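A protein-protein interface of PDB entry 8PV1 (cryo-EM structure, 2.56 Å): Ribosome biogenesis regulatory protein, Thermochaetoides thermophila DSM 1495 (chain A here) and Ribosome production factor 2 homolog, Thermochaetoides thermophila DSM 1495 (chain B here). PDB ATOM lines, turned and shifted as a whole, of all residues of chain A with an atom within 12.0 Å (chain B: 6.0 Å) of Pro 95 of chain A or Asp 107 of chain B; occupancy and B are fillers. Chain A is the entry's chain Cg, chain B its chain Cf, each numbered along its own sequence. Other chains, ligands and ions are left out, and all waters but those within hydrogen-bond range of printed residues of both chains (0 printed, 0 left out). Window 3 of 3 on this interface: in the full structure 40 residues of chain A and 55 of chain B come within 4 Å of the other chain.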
ATOM      1  N   LEU A  90      -4.976  36.628  18.662  1.00  0.00           N
ATOM      2  CA  LEU A  90      -5.516  36.065  19.889  1.00  0.00           C
ATOM      3  C   LEU A  90      -5.296  34.561  19.899  1.00  0.00           C
ATOM      4  O   LEU A  90      -5.371  33.914  18.848  1.00  0.00           O
ATOM      5  CB  LEU A  90      -7.015  36.372  20.030  1.00  0.00           C
ATOM      6  CG  LEU A  90      -7.351  37.821  20.381  1.00  0.00           C
ATOM      7  CD1 LEU A  90      -8.757  38.159  19.940  1.00  0.00           C
ATOM      8  CD2 LEU A  90      -7.189  38.057  21.872  1.00  0.00           C
ATOM      9  N   PRO A  91      -5.020  33.979  21.067  1.00  0.00           N
ATOM     10  CA  PRO A  91      -4.736  32.541  21.118  1.00  0.00           C
ATOM     11  C   PRO A  91      -5.993  31.702  20.956  1.00  0.00           C
ATOM     12  O   PRO A  91      -7.079  32.077  21.403  1.00  0.00           O
ATOM     13  CB  PRO A  91      -4.119  32.352  22.508  1.00  0.00           C
ATOM     14  CG  PRO A  91      -4.667  33.469  23.311  1.00  0.00           C
ATOM     15  CD  PRO A  91      -4.811  34.628  22.372  1.00  0.00           C
ATOM     16  N   ARG A  92      -5.831  30.555  20.305  1.00  0.00           N
ATOM     17  CA  ARG A  92      -6.899  29.576  20.208  1.00  0.00           C
ATOM     18  C   ARG A  92      -7.054  28.835  21.531  1.00  0.00           C
ATOM     19  O   ARG A  92      -6.154  28.820  22.375  1.00  0.00           O
ATOM     20  CB  ARG A  92      -6.617  28.580  19.082  1.00  0.00           C
ATOM     21  CG  ARG A  92      -6.878  29.115  17.687  1.00  0.00           C
ATOM     22  CD  ARG A  92      -6.362  28.155  16.629  1.00  0.00           C
ATOM     23  NE  ARG A  92      -6.895  26.810  16.803  1.00  0.00           N
ATOM     24  CZ  ARG A  92      -7.951  26.332  16.157  1.00  0.00           C
ATOM     25  NH1 ARG A  92      -8.613  27.065  15.279  1.00  0.00           N
ATOM     26  NH2 ARG A  92      -8.350  25.087  16.400  1.00  0.00           N
ATOM     27  N   GLU A  93      -8.219  28.218  21.710  1.00  0.00           N
ATOM     28  CA  GLU A  93      -8.462  27.415  22.900  1.00  0.00           C
ATOM     29  C   GLU A  93      -8.072  25.957  22.711  1.00  0.00           C
ATOM     30  O   GLU A  93      -7.815  25.259  23.697  1.00  0.00           O
ATOM     31  CB  GLU A  93      -9.934  27.508  23.311  1.00  0.00           C
ATOM     32  CG  GLU A  93     -10.910  26.908  22.316  1.00  0.00           C
ATOM     33  CD  GLU A  93     -12.352  27.083  22.739  1.00  0.00           C
ATOM     34  OE1 GLU A  93     -12.590  27.695  23.801  1.00  0.00           O
ATOM     35  OE2 GLU A  93     -13.248  26.611  22.010  1.00  0.00           O
ATOM     36  N   LYS A  94      -8.028  25.485  21.471  1.00  0.00           N
ATOM     37  CA  LYS A  94      -7.681  24.118  21.127  1.00  0.00           C
ATOM     38  C   LYS A  94      -6.750  24.123  19.925  1.00  0.00           C
ATOM     39  O   LYS A  94      -6.767  25.073  19.134  1.00  0.00           O
ATOM     40  CB  LYS A  94      -8.940  23.293  20.818  1.00  0.00           C
ATOM     41  CG  LYS A  94      -9.798  22.999  22.037  1.00  0.00           C
ATOM     42  CD  LYS A  94     -11.187  22.538  21.644  1.00  0.00           C
ATOM     43  CE  LYS A  94     -12.100  22.458  22.853  1.00  0.00           C
ATOM     44  NZ  LYS A  94     -13.507  22.186  22.458  1.00  0.00           N
ATOM     45  N   PRO A  95      -5.912  23.096  19.774  1.00  0.00           N
ATOM     46  CA  PRO A  95      -5.000  23.057  18.624  1.00  0.00           C
ATOM     47  C   PRO A  95      -5.746  22.897  17.309  1.00  0.00           C
ATOM     48  O   PRO A  95      -6.894  22.448  17.268  1.00  0.00           O
ATOM     49  CB  PRO A  95      -4.111  21.840  18.912  1.00  0.00           C
ATOM     50  CG  PRO A  95      -4.835  21.058  19.949  1.00  0.00           C
ATOM     51  CD  PRO A  95      -5.583  22.055  20.760  1.00  0.00           C
ATOM     52  N   VAL A  96      -5.078  23.305  16.232  1.00  0.00           N
ATOM     53  CA  VAL A  96      -5.640  23.210  14.879  1.00  0.00           C
ATOM     54  C   VAL A  96      -5.866  21.743  14.538  1.00  0.00           C
ATOM     55  O   VAL A  96      -5.009  20.897  14.868  1.00  0.00           O
ATOM     56  CB  VAL A  96      -4.696  23.881  13.865  1.00  0.00           C
ATOM     57  CG1 VAL A  96      -5.128  23.620  12.429  1.00  0.00           C
ATOM     58  CG2 VAL A  96      -4.614  25.375  14.131  1.00  0.00           C
ATOM     59  N   PRO A  97      -7.006  21.373  13.949  1.00  0.00           N
ATOM     60  CA  PRO A  97      -7.245  19.966  13.595  1.00  0.00           C
ATOM     61  C   PRO A  97      -6.215  19.443  12.604  1.00  0.00           C
ATOM     62  O   PRO A  97      -5.774  20.154  11.700  1.00  0.00           O
ATOM     63  CB  PRO A  97      -8.649  19.990  12.984  1.00  0.00           C
ATOM     64  CG  PRO A  97      -9.298  21.180  13.578  1.00  0.00           C
ATOM     65  CD  PRO A  97      -8.213  22.198  13.768  1.00  0.00           C
ATOM     66  N   GLN A  98      -5.838  18.186  12.788  1.00  0.00           N
ATOM     67  CA  GLN A  98      -4.827  17.509  11.998  1.00  0.00           C
ATOM     68  C   GLN A  98      -5.432  16.259  11.377  1.00  0.00           C
ATOM     69  O   GLN A  98      -6.432  15.732  11.880  1.00  0.00           O
ATOM     70  CB  GLN A  98      -3.621  17.131  12.871  1.00  0.00           C
ATOM     71  CG  GLN A  98      -2.860  18.322  13.427  1.00  0.00           C
ATOM     72  CD  GLN A  98      -2.250  19.185  12.341  1.00  0.00           C
ATOM     73  OE1 GLN A  98      -2.696  20.305  12.097  1.00  0.00           O
ATOM     74  NE2 GLN A  98      -1.221  18.666  11.683  1.00  0.00           N
ATOM     75  N   PRO A  99      -4.884  15.784  10.256  1.00  0.00           N
ATOM     76  CA  PRO A  99      -5.354  14.512   9.694  1.00  0.00           C
ATOM     77  C   PRO A  99      -5.110  13.353  10.650  1.00  0.00           C
ATOM     78  O   PRO A  99      -4.103  13.309  11.360  1.00  0.00           O
ATOM     79  CB  PRO A  99      -4.531  14.367   8.410  1.00  0.00           C
ATOM     80  CG  PRO A  99      -4.166  15.761   8.043  1.00  0.00           C
ATOM     81  CD  PRO A  99      -3.951  16.471   9.346  1.00  0.00           C
ATOM     82  N   LYS A 100      -6.055  12.419  10.666  1.00  0.00           N
ATOM     83  CA  LYS A 100      -5.964  11.268  11.546  1.00  0.00           C
ATOM     84  C   LYS A 100      -4.848  10.335  11.075  1.00  0.00           C
ATOM     85  O   LYS A 100      -4.455  10.373   9.906  1.00  0.00           O
ATOM     86  CB  LYS A 100      -7.293  10.510  11.585  1.00  0.00           C
ATOM     87  CG  LYS A 100      -8.352  11.065  12.543  1.00  0.00           C
ATOM     88  CD  LYS A 100      -8.995  12.352  12.047  1.00  0.00           C
ATOM     89  CE  LYS A 100      -9.874  12.096  10.833  1.00  0.00           C
ATOM     90  NZ  LYS A 100     -10.560  13.334  10.373  1.00  0.00           N
ATOM     91  N   PRO B  21     -11.857  19.596  18.603  1.00  0.00           N
ATOM     92  CA  PRO B  21     -11.216  20.747  17.952  1.00  0.00           C
ATOM     93  C   PRO B  21     -11.796  21.012  16.570  1.00  0.00           C
ATOM     94  O   PRO B  21     -12.148  20.089  15.834  1.00  0.00           O
ATOM     95  CB  PRO B  21      -9.745  20.331  17.872  1.00  0.00           C
ATOM     96  CG  PRO B  21      -9.575  19.355  18.977  1.00  0.00           C
ATOM     97  CD  PRO B  21     -10.865  18.595  19.036  1.00  0.00           C
ATOM     98  N   LYS B  22     -11.889  22.294  16.220  1.00  0.00           N
ATOM     99  CA  LYS B  22     -12.495  22.720  14.967  1.00  0.00           C
ATOM    100  C   LYS B  22     -11.616  23.770  14.307  1.00  0.00           C
ATOM    101  O   LYS B  22     -10.783  24.410  14.953  1.00  0.00           O
ATOM    102  CB  LYS B  22     -13.907  23.286  15.180  1.00  0.00           C
ATOM    103  CG  LYS B  22     -14.905  22.300  15.762  1.00  0.00           C
ATOM    104  CD  LYS B  22     -16.165  23.002  16.227  1.00  0.00           C
ATOM    105  CE  LYS B  22     -17.127  22.025  16.877  1.00  0.00           C
ATOM    106  NZ  LYS B  22     -18.357  22.701  17.367  1.00  0.00           N
ATOM    107  N   GLU B  25     -13.306  27.934  15.740  1.00  0.00           N
ATOM    108  CA  GLU B  25     -13.542  27.572  17.125  1.00  0.00           C
ATOM    109  C   GLU B  25     -14.841  28.183  17.643  1.00  0.00           C
ATOM    110  O   GLU B  25     -15.321  29.209  17.155  1.00  0.00           O
ATOM    111  CB  GLU B  25     -12.376  28.019  18.003  1.00  0.00           C
ATOM    112  CG  GLU B  25     -11.130  27.170  17.859  1.00  0.00           C
ATOM    113  CD  GLU B  25     -10.087  27.500  18.903  1.00  0.00           C
ATOM    114  OE1 GLU B  25     -10.021  28.673  19.326  1.00  0.00           O
ATOM    115  OE2 GLU B  25      -9.337  26.587  19.306  1.00  0.00           O
ATOM    116  N   GLU B  80     -10.875  20.597  31.674  1.00  0.00           N
ATOM    117  CA  GLU B  80     -11.234  19.356  30.992  1.00  0.00           C
ATOM    118  C   GLU B  80     -12.706  19.012  31.179  1.00  0.00           C
ATOM    119  O   GLU B  80     -13.390  18.647  30.216  1.00  0.00           O
ATOM    120  CB  GLU B  80     -10.361  18.213  31.517  1.00  0.00           C
ATOM    121  CG  GLU B  80     -10.710  16.835  30.972  1.00  0.00           C
ATOM    122  CD  GLU B  80     -10.391  16.676  29.505  1.00  0.00           C
ATOM    123  OE1 GLU B  80      -9.454  17.344  29.029  1.00  0.00           O
ATOM    124  OE2 GLU B  80     -11.079  15.884  28.827  1.00  0.00           O
ATOM    125  N   MET B 105      -6.384  28.991  29.184  1.00  0.00           N
ATOM    126  CA  MET B 105      -6.003  27.615  28.910  1.00  0.00           C
ATOM    127  C   MET B 105      -5.674  27.434  27.436  1.00  0.00           C
ATOM    128  O   MET B 105      -6.027  28.265  26.595  1.00  0.00           O
ATOM    129  CB  MET B 105      -7.134  26.638  29.269  1.00  0.00           C
ATOM    130  CG  MET B 105      -7.509  26.539  30.736  1.00  0.00           C
ATOM    131  SD  MET B 105      -6.186  25.898  31.769  1.00  0.00           S
ATOM    132  CE  MET B 105      -6.882  26.141  33.397  1.00  0.00           C
ATOM    133  N   PHE B 106      -4.992  26.331  27.134  1.00  0.00           N
ATOM    134  CA  PHE B 106      -4.849  25.840  25.772  1.00  0.00           C
ATOM    135  C   PHE B 106      -4.728  24.327  25.820  1.00  0.00           C
ATOM    136  O   PHE B 106      -3.823  23.804  26.476  1.00  0.00           O
ATOM    137  CB  PHE B 106      -3.633  26.445  25.063  1.00  0.00           C
ATOM    138  CG  PHE B 106      -3.394  25.878  23.691  1.00  0.00           C
ATOM    139  CD1 PHE B 106      -4.225  26.215  22.637  1.00  0.00           C
ATOM    140  CD2 PHE B 106      -2.345  25.005  23.458  1.00  0.00           C
ATOM    141  CE1 PHE B 106      -4.015  25.692  21.376  1.00  0.00           C
ATOM    142  CE2 PHE B 106      -2.129  24.479  22.198  1.00  0.00           C
ATOM    143  CZ  PHE B 106      -2.965  24.825  21.157  1.00  0.00           C
ATOM    144  N   ASP B 107      -5.637  23.642  25.116  1.00  0.00           N
ATOM    145  CA  ASP B 107      -5.706  22.177  25.074  1.00  0.00           C
ATOM    146  C   ASP B 107      -5.818  21.581  26.475  1.00  0.00           C
ATOM    147  O   ASP B 107      -5.134  20.611  26.814  1.00  0.00           O
ATOM    148  CB  ASP B 107      -4.511  21.585  24.320  1.00  0.00           C
ATOM    149  CG  ASP B 107      -4.822  20.239  23.703  1.00  0.00           C
ATOM    150  OD1 ASP B 107      -6.000  19.826  23.735  1.00  0.00           O
ATOM    151  OD2 ASP B 107      -3.887  19.594  23.184  1.00  0.00           O
ATOM    152  N   TYR B 108      -6.677  22.195  27.299  1.00  0.00           N
ATOM    153  CA  TYR B 108      -6.951  21.776  28.679  1.00  0.00           C
ATOM    154  C   TYR B 108      -5.697  21.791  29.550  1.00  0.00           C
ATOM    155  O   TYR B 108      -5.587  21.034  30.516  1.00  0.00           O
ATOM    156  CB  TYR B 108      -7.630  20.403  28.719  1.00  0.00           C
ATOM    157  CG  TYR B 108      -8.820  20.307  27.794  1.00  0.00           C
ATOM    158  CD1 TYR B 108      -9.900  21.169  27.935  1.00  0.00           C
ATOM    159  CD2 TYR B 108      -8.850  19.383  26.758  1.00  0.00           C
ATOM    160  CE1 TYR B 108     -10.988  21.094  27.090  1.00  0.00           C
ATOM    161  CE2 TYR B 108      -9.935  19.301  25.909  1.00  0.00           C
ATOM    162  CZ  TYR B 108     -10.999  20.160  26.078  1.00  0.00           C
ATOM    163  OH  TYR B 108     -12.080  20.084  25.233  1.00  0.00           O
ATOM    164  N   LYS B 109      -4.746  22.660  29.212  1.00  0.00           N
ATOM    165  CA  LYS B 109      -3.560  22.896  30.019  1.00  0.00           C
ATOM    166  C   LYS B 109      -3.370  24.397  30.147  1.00  0.00           C
ATOM    167  O   LYS B 109      -3.825  25.164  29.296  1.00  0.00           O
ATOM    168  CB  LYS B 109      -2.308  22.254  29.410  1.00  0.00           C
ATOM    169  CG  LYS B 109      -2.325  20.736  29.394  1.00  0.00           C
ATOM    170  CD  LYS B 109      -0.984  20.183  28.947  1.00  0.00           C
ATOM    171  CE  LYS B 109      -0.766  20.402  27.461  1.00  0.00           C
ATOM    172  NZ  LYS B 109       0.506  19.789  26.990  1.00  0.00           N
ATOM    173  N   GLU B 270       1.894  27.043  18.954  1.00  0.00           N
ATOM    174  CA  GLU B 270       0.772  26.193  18.563  1.00  0.00           C
ATOM    175  C   GLU B 270      -0.571  26.873  18.802  1.00  0.00           C
ATOM    176  O   GLU B 270      -1.505  26.688  18.013  1.00  0.00           O
ATOM    177  CB  GLU B 270       0.827  24.861  19.310  1.00  0.00           C
ATOM    178  CG  GLU B 270       2.059  24.030  19.012  1.00  0.00           C
ATOM    179  CD  GLU B 270       2.250  22.901  20.004  1.00  0.00           C
ATOM    180  OE1 GLU B 270       1.504  22.856  21.005  1.00  0.00           O
ATOM    181  OE2 GLU B 270       3.145  22.058  19.784  1.00  0.00           O
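Of chain A, only Glu 93 and Pro 95 come within 4 Å of Asp 107 of chain B. Pro 21 of chain B touches two residues of chain A. Phe 106 of chain B touches just these residues of chain A: Arg 92, Glu 93, Lys 94 and Pro 95. Of chain A, only Lys 94 comes within 4 Å of Tyr 108 of chain B. No residue of chain A comes within 4 Å of Glu 270 of chain B. Of the printed residues of chain B, Lys 94 of chain A touches Glu 25 (2.8 Å), Phe 106 (3.5 Å) and Tyr 108 (3.4 Å). Printed residues of chain B within 4 Å of Arg 92 of chain A: Lys 22, Glu 25 and Phe 106. Of the printed residues of chain A, Lys 22 of chain B touches Arg 92 and Pro 97. Lys 100 of chain A touches none of the printed residues of chain B. Met 105 of chain B touches none of the printed residues of chain A. The nearest residue of chain A that does not touch Asp 107 of chain B is Lys 94 of chain A (4.5 Å).
The backbone carbonyl oxygen of Lys 94 of chain A lies within hydrogen-bond range of the guanidinium group of Arg 92 of chain A (2.9 Å). O of Pro 95 of chain A sits at hydrogen-bond distance from NH2 of Arg 92 of chain A (3.1 Å).
The guanidinium group of Arg 92 of chain A lies within hydrogen-bond range of the backbone carbonyl oxygen of Lys 22 of chain B, at 2.9 Å. The guanidinium group (NH2) of Arg 92 of chain A is in salt-bridge range of the side-chain carboxylate (OE2) of Glu 25 of chain B, at 3.4 Å. The side-chain carboxylate of Glu 25 of chain B is in hydrogen-bond range of the backbone NH of Glu 93 of chain A (3.0 Å). OE2 of Glu 25 of chain B sits at hydrogen-bond distance from N of Lys 94 of chain A (2.8 Å). The backbone NH (N) of Asp 107 of chain B sits at hydrogen-bond distance from the backbone carbonyl oxygen (O) of Glu 93 of chain A, at 3.1 Å.
Of the 11 printed residues of chain A, 5 touch a printed residue of chain B. Hydrophobic or aromatic side chains of chain A within 4 Å of the printed part of chain B: Pro 95 and Pro 97. Among the printed residues, Asp or Glu carboxylates within 4 Å of a Lys or Arg side-chain nitrogen of the other chain: Arg 92 of chain A with Glu 25 of chain B (3.4 Å).
Arg 92 of chain A touches Phe 106 of chain B. Glu 93 of chain A touches Phe 106 of chain B. CE1 of Phe 106 of chain B touches C of Lys 94 of chain A (3.5 Å). Tyr 108 of chain B touches Lys 94 of chain A. Pro 95 of chain A touches Pro 21 of chain B (O to CB, 3.6 Å). Pro 95 of chain A touches Phe 106 of chain B. CG of Asp 107 of chain B touches CD of Pro 95 of chain A, at 3.5 Å. Pro 21 of chain B touches Pro 97 of chain A. Lys 22 of chain B touches Pro 97 of chain A.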
